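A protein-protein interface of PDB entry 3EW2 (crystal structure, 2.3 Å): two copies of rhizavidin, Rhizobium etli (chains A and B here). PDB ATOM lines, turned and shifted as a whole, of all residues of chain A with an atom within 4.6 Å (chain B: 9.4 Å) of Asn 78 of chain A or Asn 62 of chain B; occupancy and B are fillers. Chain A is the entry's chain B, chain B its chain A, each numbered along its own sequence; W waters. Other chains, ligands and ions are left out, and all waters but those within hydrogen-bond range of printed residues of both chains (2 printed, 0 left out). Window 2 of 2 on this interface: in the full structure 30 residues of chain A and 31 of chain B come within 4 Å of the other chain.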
ATOM      1  N   CYS A  50      -0.942  19.426 -31.530  1.00  0.00           N
ATOM      2  CA  CYS A  50      -0.136  19.805 -30.358  1.00  0.00           C
ATOM      3  C   CYS A  50       0.363  21.271 -30.311  1.00  0.00           C
ATOM      4  O   CYS A  50       1.511  21.520 -29.957  1.00  0.00           O
ATOM      5  CB  CYS A  50       1.042  18.821 -30.180  1.00  0.00           C
ATOM      6  SG  CYS A  50       0.415  17.212 -29.726  1.00  0.00           S
ATOM      7  N   GLY A  71       9.170  15.262 -26.894  1.00  0.00           N
ATOM      8  CA  GLY A  71       8.130  14.256 -27.173  1.00  0.00           C
ATOM      9  C   GLY A  71       6.784  14.907 -27.114  1.00  0.00           C
ATOM     10  O   GLY A  71       6.542  15.716 -26.214  1.00  0.00           O
ATOM     11  N   TRP A  72       5.887  14.563 -28.041  1.00  0.00           N
ATOM     12  CA  TRP A  72       4.651  15.332 -28.183  1.00  0.00           C
ATOM     13  C   TRP A  72       3.522  14.775 -27.322  1.00  0.00           C
ATOM     14  O   TRP A  72       2.425  14.454 -27.814  1.00  0.00           O
ATOM     15  CB  TRP A  72       4.264  15.564 -29.662  1.00  0.00           C
ATOM     16  CG  TRP A  72       5.316  16.362 -30.422  1.00  0.00           C
ATOM     17  CD1 TRP A  72       6.175  15.885 -31.374  1.00  0.00           C
ATOM     18  CD2 TRP A  72       5.636  17.777 -30.266  1.00  0.00           C
ATOM     19  NE1 TRP A  72       7.004  16.904 -31.823  1.00  0.00           N
ATOM     20  CE2 TRP A  72       6.689  18.068 -31.168  1.00  0.00           C
ATOM     21  CE3 TRP A  72       5.104  18.821 -29.475  1.00  0.00           C
ATOM     22  CZ2 TRP A  72       7.262  19.355 -31.281  1.00  0.00           C
ATOM     23  CZ3 TRP A  72       5.638  20.087 -29.594  1.00  0.00           C
ATOM     24  CH2 TRP A  72       6.735  20.346 -30.489  1.00  0.00           C
ATOM     25  N   ASN A  73       3.815  14.652 -26.034  1.00  0.00           N
ATOM     26  CA  ASN A  73       2.785  14.451 -25.017  1.00  0.00           C
ATOM     27  C   ASN A  73       3.111  15.251 -23.766  1.00  0.00           C
ATOM     28  O   ASN A  73       4.197  15.130 -23.214  1.00  0.00           O
ATOM     29  CB  ASN A  73       2.605  12.965 -24.679  1.00  0.00           C
ATOM     30  CG  ASN A  73       1.362  12.696 -23.782  1.00  0.00           C
ATOM     31  OD1 ASN A  73       0.496  13.574 -23.556  1.00  0.00           O
ATOM     32  ND2 ASN A  73       1.277  11.474 -23.271  1.00  0.00           N
ATOM     33  N   THR A  76      -2.004  17.507 -21.946  1.00  0.00           N
ATOM     34  CA  THR A  76      -3.056  18.369 -22.496  1.00  0.00           C
ATOM     35  C   THR A  76      -3.368  17.867 -23.886  1.00  0.00           C
ATOM     36  O   THR A  76      -4.519  17.876 -24.310  1.00  0.00           O
ATOM     37  CB  THR A  76      -2.590  19.822 -22.604  1.00  0.00           C
ATOM     38  OG1 THR A  76      -2.295  20.320 -21.299  1.00  0.00           O
ATOM     39  CG2 THR A  76      -3.652  20.706 -23.271  1.00  0.00           C
ATOM     40  N   GLU A  77      -2.340  17.436 -24.605  1.00  0.00           N
ATOM     41  CA  GLU A  77      -2.537  16.890 -25.940  1.00  0.00           C
ATOM     42  C   GLU A  77      -1.407  15.969 -26.291  1.00  0.00           C
ATOM     43  O   GLU A  77      -0.230  16.312 -26.111  1.00  0.00           O
ATOM     44  CB  GLU A  77      -2.648  18.005 -26.987  1.00  0.00           C
ATOM     45  CG  GLU A  77      -3.024  17.527 -28.346  1.00  0.00           C
ATOM     46  CD  GLU A  77      -3.538  18.654 -29.259  1.00  0.00           C
ATOM     47  OE1 GLU A  77      -4.139  19.630 -28.758  1.00  0.00           O
ATOM     48  OE2 GLU A  77      -3.363  18.555 -30.488  1.00  0.00           O
ATOM     49  N   ASN A  78      -1.789  14.799 -26.795  1.00  0.00           N
ATOM     50  CA  ASN A  78      -0.843  13.801 -27.277  1.00  0.00           C
ATOM     51  C   ASN A  78      -0.936  13.565 -28.777  1.00  0.00           C
ATOM     52  O   ASN A  78      -1.967  13.061 -29.272  1.00  0.00           O
ATOM     53  CB  ASN A  78      -1.038  12.467 -26.508  1.00  0.00           C
ATOM     54  CG  ASN A  78      -0.050  11.351 -26.979  1.00  0.00           C
ATOM     55  OD1 ASN A  78       0.954  11.640 -27.613  1.00  0.00           O
ATOM     56  ND2 ASN A  78      -0.380  10.084 -26.698  1.00  0.00           N
ATOM     57  N   CYS A  79       0.150  13.852 -29.490  1.00  0.00           N
ATOM     58  CA  CYS A  79       0.180  13.667 -30.953  1.00  0.00           C
ATOM     59  C   CYS A  79       0.938  12.423 -31.396  1.00  0.00           C
ATOM     60  O   CYS A  79       1.272  12.272 -32.579  1.00  0.00           O
ATOM     61  CB  CYS A  79       0.790  14.903 -31.657  1.00  0.00           C
ATOM     62  SG  CYS A  79      -0.216  16.422 -31.510  1.00  0.00           S
ATOM     63  N   ASN A  80       1.254  11.556 -30.446  1.00  0.00           N
ATOM     64  CA  ASN A  80       1.931  10.297 -30.738  1.00  0.00           C
ATOM     65  C   ASN A  80       3.133  10.458 -31.678  1.00  0.00           C
ATOM     66  O   ASN A  80       3.142   9.915 -32.772  1.00  0.00           O
ATOM     67  CB  ASN A  80       0.906   9.311 -31.276  1.00  0.00           C
ATOM     68  CG  ASN A  80       1.386   7.911 -31.234  1.00  0.00           C
ATOM     69  OD1 ASN A  80       1.933   7.448 -30.210  1.00  0.00           O
ATOM     70  ND2 ASN A  80       1.214   7.201 -32.353  1.00  0.00           N
ATOM     71  N   SER A  81       4.144  11.210 -31.235  1.00  0.00           N
ATOM     72  CA  SER A  81       5.225  11.647 -32.084  1.00  0.00           C
ATOM     73  C   SER A  81       6.316  12.283 -31.255  1.00  0.00           C
ATOM     74  O   SER A  81       6.119  12.560 -30.067  1.00  0.00           O
ATOM     75  CB  SER A  81       4.750  12.711 -33.104  1.00  0.00           C
ATOM     76  OG  SER A  81       4.386  13.919 -32.470  1.00  0.00           O
ATOM     77  N   VAL B  31      15.113   5.298 -19.581  1.00  0.00           N
ATOM     78  CA  VAL B  31      13.898   6.054 -19.652  1.00  0.00           C
ATOM     79  C   VAL B  31      13.390   6.209 -18.235  1.00  0.00           C
ATOM     80  O   VAL B  31      13.130   5.206 -17.570  1.00  0.00           O
ATOM     81  CB  VAL B  31      12.808   5.297 -20.435  1.00  0.00           C
ATOM     82  CG1 VAL B  31      11.440   5.960 -20.201  1.00  0.00           C
ATOM     83  CG2 VAL B  31      13.095   5.282 -21.926  1.00  0.00           C
ATOM     84  N   PHE B  34       9.287  10.259 -15.990  1.00  0.00           N
ATOM     85  CA  PHE B  34       8.743  11.461 -16.625  1.00  0.00           C
ATOM     86  C   PHE B  34       8.872  11.487 -18.146  1.00  0.00           C
ATOM     87  O   PHE B  34       8.587  12.488 -18.749  1.00  0.00           O
ATOM     88  CB  PHE B  34       9.408  12.697 -16.050  1.00  0.00           C
ATOM     89  CG  PHE B  34       9.531  12.674 -14.558  1.00  0.00           C
ATOM     90  CD1 PHE B  34      10.776  12.407 -13.952  1.00  0.00           C
ATOM     91  CD2 PHE B  34       8.421  12.925 -13.748  1.00  0.00           C
ATOM     92  CE1 PHE B  34      10.902  12.392 -12.561  1.00  0.00           C
ATOM     93  CE2 PHE B  34       8.539  12.909 -12.358  1.00  0.00           C
ATOM     94  CZ  PHE B  34       9.781  12.642 -11.762  1.00  0.00           C
ATOM     95  N   GLY B  35       9.300  10.382 -18.744  1.00  0.00           N
ATOM     96  CA  GLY B  35       9.593  10.296 -20.183  1.00  0.00           C
ATOM     97  C   GLY B  35      10.925  10.879 -20.631  1.00  0.00           C
ATOM     98  O   GLY B  35      11.127  11.065 -21.824  1.00  0.00           O
ATOM     99  N   ASN B  36      11.827  11.192 -19.700  1.00  0.00           N
ATOM    100  CA  ASN B  36      13.215  11.564 -20.052  1.00  0.00           C
ATOM    101  C   ASN B  36      14.121  10.378 -20.480  1.00  0.00           C
ATOM    102  O   ASN B  36      13.974   9.268 -19.995  1.00  0.00           O
ATOM    103  CB  ASN B  36      13.916  12.306 -18.901  1.00  0.00           C
ATOM    104  CG  ASN B  36      13.218  13.615 -18.494  1.00  0.00           C
ATOM    105  OD1 ASN B  36      13.127  14.575 -19.267  1.00  0.00           O
ATOM    106  ND2 ASN B  36      12.749  13.659 -17.258  1.00  0.00           N
ATOM    107  N   VAL B  37      15.086  10.638 -21.366  1.00  0.00           N
ATOM    108  CA  VAL B  37      16.048   9.622 -21.777  1.00  0.00           C
ATOM    109  C   VAL B  37      17.404  10.123 -21.360  1.00  0.00           C
ATOM    110  O   VAL B  37      17.731  11.301 -21.521  1.00  0.00           O
ATOM    111  CB  VAL B  37      16.009   9.330 -23.309  1.00  0.00           C
ATOM    112  CG1 VAL B  37      17.014   8.234 -23.706  1.00  0.00           C
ATOM    113  CG2 VAL B  37      14.635   8.902 -23.708  1.00  0.00           C
ATOM    114  N   GLY B  59      17.324  12.919 -24.078  1.00  0.00           N
ATOM    115  CA  GLY B  59      16.232  12.815 -25.016  1.00  0.00           C
ATOM    116  C   GLY B  59      14.865  12.764 -24.373  1.00  0.00           C
ATOM    117  O   GLY B  59      14.711  12.941 -23.139  1.00  0.00           O
ATOM    118  N   ARG B  60      13.862  12.481 -25.203  1.00  0.00           N
ATOM    119  CA  ARG B  60      12.495  12.336 -24.723  1.00  0.00           C
ATOM    120  C   ARG B  60      11.851  11.184 -25.442  1.00  0.00           C
ATOM    121  O   ARG B  60      12.176  10.927 -26.580  1.00  0.00           O
ATOM    122  CB  ARG B  60      11.665  13.644 -24.968  1.00  0.00           C
ATOM    123  CG  ARG B  60      12.195  14.923 -24.278  1.00  0.00           C
ATOM    124  CD  ARG B  60      11.796  15.011 -22.798  1.00  0.00           C
ATOM    125  NE  ARG B  60      10.368  14.727 -22.650  1.00  0.00           N
ATOM    126  CZ  ARG B  60       9.732  14.502 -21.503  1.00  0.00           C
ATOM    127  NH1 ARG B  60      10.359  14.519 -20.341  1.00  0.00           N
ATOM    128  NH2 ARG B  60       8.424  14.246 -21.525  1.00  0.00           N
ATOM    129  N   VAL B  61      10.899  10.530 -24.802  1.00  0.00           N
ATOM    130  CA  VAL B  61      10.139   9.442 -25.418  1.00  0.00           C
ATOM    131  C   VAL B  61       8.669   9.753 -25.373  1.00  0.00           C
ATOM    132  O   VAL B  61       8.200  10.436 -24.455  1.00  0.00           O
ATOM    133  CB  VAL B  61      10.267   8.100 -24.636  1.00  0.00           C
ATOM    134  CG1 VAL B  61      10.982   7.068 -25.451  1.00  0.00           C
ATOM    135  CG2 VAL B  61      10.970   8.294 -23.261  1.00  0.00           C
ATOM    136  N   ASN B  62       7.928   9.225 -26.334  1.00  0.00           N
ATOM    137  CA  ASN B  62       6.486   9.399 -26.377  1.00  0.00           C
ATOM    138  C   ASN B  62       5.925   8.129 -26.961  1.00  0.00           C
ATOM    139  O   ASN B  62       6.016   7.919 -28.147  1.00  0.00           O
ATOM    140  CB  ASN B  62       6.149  10.635 -27.253  1.00  0.00           C
ATOM    141  CG  ASN B  62       4.644  10.916 -27.348  1.00  0.00           C
ATOM    142  OD1 ASN B  62       3.816  10.155 -26.871  1.00  0.00           O
ATOM    143  ND2 ASN B  62       4.302  12.025 -27.965  1.00  0.00           N
ATOM    144  N   GLY B  63       5.407   7.244 -26.130  1.00  0.00           N
ATOM    145  CA  GLY B  63       4.874   5.992 -26.650  1.00  0.00           C
ATOM    146  C   GLY B  63       5.981   5.255 -27.393  1.00  0.00           C
ATOM    147  O   GLY B  63       7.053   4.984 -26.847  1.00  0.00           O
ATOM    148  N   THR B  64       5.770   4.999 -28.666  1.00  0.00           N
ATOM    149  CA  THR B  64       6.764   4.240 -29.370  1.00  0.00           C
ATOM    150  C   THR B  64       7.809   5.092 -30.116  1.00  0.00           C
ATOM    151  O   THR B  64       8.630   4.540 -30.818  1.00  0.00           O
ATOM    152  CB  THR B  64       6.063   3.208 -30.259  1.00  0.00           C
ATOM    153  OG1 THR B  64       6.946   2.115 -30.480  1.00  0.00           O
ATOM    154  CG2 THR B  64       5.641   3.780 -31.569  1.00  0.00           C
ATOM    155  N   PHE B  65       7.781   6.426 -29.921  1.00  0.00           N
ATOM    156  CA  PHE B  65       8.592   7.415 -30.662  1.00  0.00           C
ATOM    157  C   PHE B  65       9.594   8.045 -29.714  1.00  0.00           C
ATOM    158  O   PHE B  65       9.344   8.061 -28.524  1.00  0.00           O
ATOM    159  CB  PHE B  65       7.679   8.522 -31.292  1.00  0.00           C
ATOM    160  CG  PHE B  65       6.782   8.004 -32.389  1.00  0.00           C
ATOM    161  CD1 PHE B  65       5.524   7.470 -32.085  1.00  0.00           C
ATOM    162  CD2 PHE B  65       7.226   7.962 -33.698  1.00  0.00           C
ATOM    163  CE1 PHE B  65       4.714   6.926 -33.091  1.00  0.00           C
ATOM    164  CE2 PHE B  65       6.414   7.383 -34.728  1.00  0.00           C
ATOM    165  CZ  PHE B  65       5.165   6.872 -34.416  1.00  0.00           C
ATOM    166  N   ILE B  66      10.685   8.622 -30.249  1.00  0.00           N
ATOM    167  CA  ILE B  66      11.791   9.067 -29.420  1.00  0.00           C
ATOM    168  C   ILE B  66      12.645  10.037 -30.194  1.00  0.00           C
ATOM    169  O   ILE B  66      12.770   9.905 -31.403  1.00  0.00           O
ATOM    170  CB  ILE B  66      12.699   7.849 -29.009  1.00  0.00           C
ATOM    171  CG1 ILE B  66      13.802   8.223 -27.993  1.00  0.00           C
ATOM    172  CG2 ILE B  66      13.283   7.130 -30.248  1.00  0.00           C
ATOM    173  CD1 ILE B  66      14.421   6.935 -27.270  1.00  0.00           C
ATOM    174  N   ALA B  67      13.218  11.000 -29.483  1.00  0.00           N
ATOM    175  CA  ALA B  67      14.240  11.848 -30.016  1.00  0.00           C
ATOM    176  C   ALA B  67      15.346  11.976 -28.957  1.00  0.00           C
ATOM    177  O   ALA B  67      15.064  12.107 -27.728  1.00  0.00           O
ATOM    178  CB  ALA B  67      13.644  13.267 -30.344  1.00  0.00           C
ATOM    179  N   GLY B  87      13.271   9.009 -34.104  1.00  0.00           N
ATOM    180  CA  GLY B  87      12.653   7.904 -34.770  1.00  0.00           C
ATOM    181  C   GLY B  87      11.601   7.198 -33.971  1.00  0.00           C
ATOM    182  O   GLY B  87      10.937   7.775 -33.103  1.00  0.00           O
ATOM    183  N   TYR B  88      11.421   5.934 -34.295  1.00  0.00           N
ATOM    184  CA  TYR B  88      10.427   5.117 -33.622  1.00  0.00           C
ATOM    185  C   TYR B  88      11.004   3.726 -33.398  1.00  0.00           C
ATOM    186  O   TYR B  88      11.809   3.259 -34.197  1.00  0.00           O
ATOM    187  CB  TYR B  88       9.191   5.046 -34.489  1.00  0.00           C
ATOM    188  CG  TYR B  88       9.469   4.653 -35.922  1.00  0.00           C
ATOM    189  CD1 TYR B  88       9.843   5.600 -36.875  1.00  0.00           C
ATOM    190  CD2 TYR B  88       9.343   3.318 -36.333  1.00  0.00           C
ATOM    191  CE1 TYR B  88      10.075   5.233 -38.192  1.00  0.00           C
ATOM    192  CE2 TYR B  88       9.599   2.931 -37.668  1.00  0.00           C
ATOM    193  CZ  TYR B  88       9.941   3.893 -38.581  1.00  0.00           C
ATOM    194  OH  TYR B  88      10.206   3.515 -39.875  1.00  0.00           O
ATOM    195  N   ALA B  89      10.621   3.079 -32.303  1.00  0.00           N
ATOM    196  CA  ALA B  89      10.929   1.663 -32.129  1.00  0.00           C
ATOM    197  C   ALA B  89       9.956   0.832 -32.941  1.00  0.00           C
ATOM    198  O   ALA B  89       8.766   1.169 -33.022  1.00  0.00           O
ATOM    199  CB  ALA B  89      10.854   1.264 -30.664  1.00  0.00           C
HETATM  200  O   HOH W   1       3.351   5.234 -29.876  1.00  0.00           O
HETATM  201  O   HOH W   2       8.766  16.459 -24.483  1.00  0.00           O
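Water W1 lies within hydrogen-bond range of OD1 of Asn 80 of chain A (2.7 Å) and N of Thr 64 of chain B (2.7 Å). Water W2 lies within hydrogen-bond range of the backbone NH (N) of Gly 71 of chain A (2.7 Å) and the guanidinium group (NE) of Arg 60 of chain B (3.0 Å).
The backbone NH (N) of Trp 72 of chain A sits close to the side-chain amide nitrogen (ND2) of Asn 62 of chain B (3.0 Å). The side-chain amide nitrogen (ND2) of Asn 62 of chain B lies close to the backbone NH (N) of Asn 73 of chain A (3.3 Å). The side-chain amide oxygen (OD1) of Asn 78 of chain A sits close to the side-chain amide oxygen (OD1) of Asn 62 of chain B, at 3.3 Å. The backbone carbonyl oxygen (O) of Ser 81 of chain A sits at hydrogen-bond distance from the side-chain amide nitrogen (ND2) of Asn 62 of chain B, at 2.8 Å.
No position is printed for both chains. Of the 9 pairs that touch across the chains among the printed residues, none has its exchanged pair printed and touching as well.
Gly 71 of chain A touches Arg 60 of chain B. Asn 62 of chain B touches Gly 71 of chain A (ND2 to C, 3.9 Å). ND2 of Asn 62 of chain B touches N of Asn 80 of chain A (3.96 Å). Asn 80 of chain A touches Phe 65 of chain B (O to CE1, 3.4 Å). Ser 81 of chain A touches Phe 65 of chain B (CA to CG, 3.97 Å).
Of the printed residues of chain B, Trp 72 of chain A touches Asn 62. Asn 78 of chain A touches just one residue of chain B: Asn 62 (3.3 Å). No residue of chain B comes within 4 Å of Cys 79 of chain A. Printed residues of chain B within 4 Å of Asn 80 of chain A: Asn 62 (3.96 Å) and Phe 65 (3.4 Å). Printed residues of chain A within 4 Å of Arg 60 of chain B: Gly 71 (3.5 Å). Asn 62 of chain B touches just these residues of chain A: Gly 71, Trp 72, Asn 73, Asn 78, Asn 80 and Ser 81. Of the printed residues of chain A, Phe 65 of chain B touches Asn 80 (3.4 Å) and Ser 81 (3.97 Å). Tyr 88 of chain B touches none of the printed residues of chain A. The nearest residue of chain B that does not touch Asn 78 of chain A is Gly 63 of chain B (6.4 Å).
Of the 10 printed residues of chain A, 6 touch a printed residue of chain B. Printed residues of chain A that touch a printed residue of chain B: Gly 71, Trp 72, Asn 73, Asn 78, Asn 80 and Ser 81. Printed residues of chain B that touch a printed residue of chain A: Arg 60, Asn 62 and Phe 65. Among the printed residues, no Asp or Glu carboxylate lies within 4 Å of a Lys or Arg side-chain nitrogen of the other chain.
The guanidinium group of Arg 60 of chain B sits at hydrogen-bond distance from the side-chain amide oxygen of Asn 36 of chain B. N of Arg 60 of chain B lies within hydrogen-bond range of O of Ala 67 of chain B (2.8 Å). The side-chain amide oxygen of Asn 78 of chain A sits close to the backbone carbonyl oxygen of Trp 72 of chain A. The backbone carbonyl oxygen (O) of Trp 72 of chain A is in hydrogen-bond range of the backbone NH (N) of Cys 79 of chain A, 2.9 Å away. The side-chain amide oxygen (OD1) of Asn 78 of chain A lies within hydrogen-bond range of the backbone NH (N) of Asn 80 of chain A. SG of Cys 50 of chain A forms a disulfide with SG of Cys 79 of chain A, 2.1 Å away.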
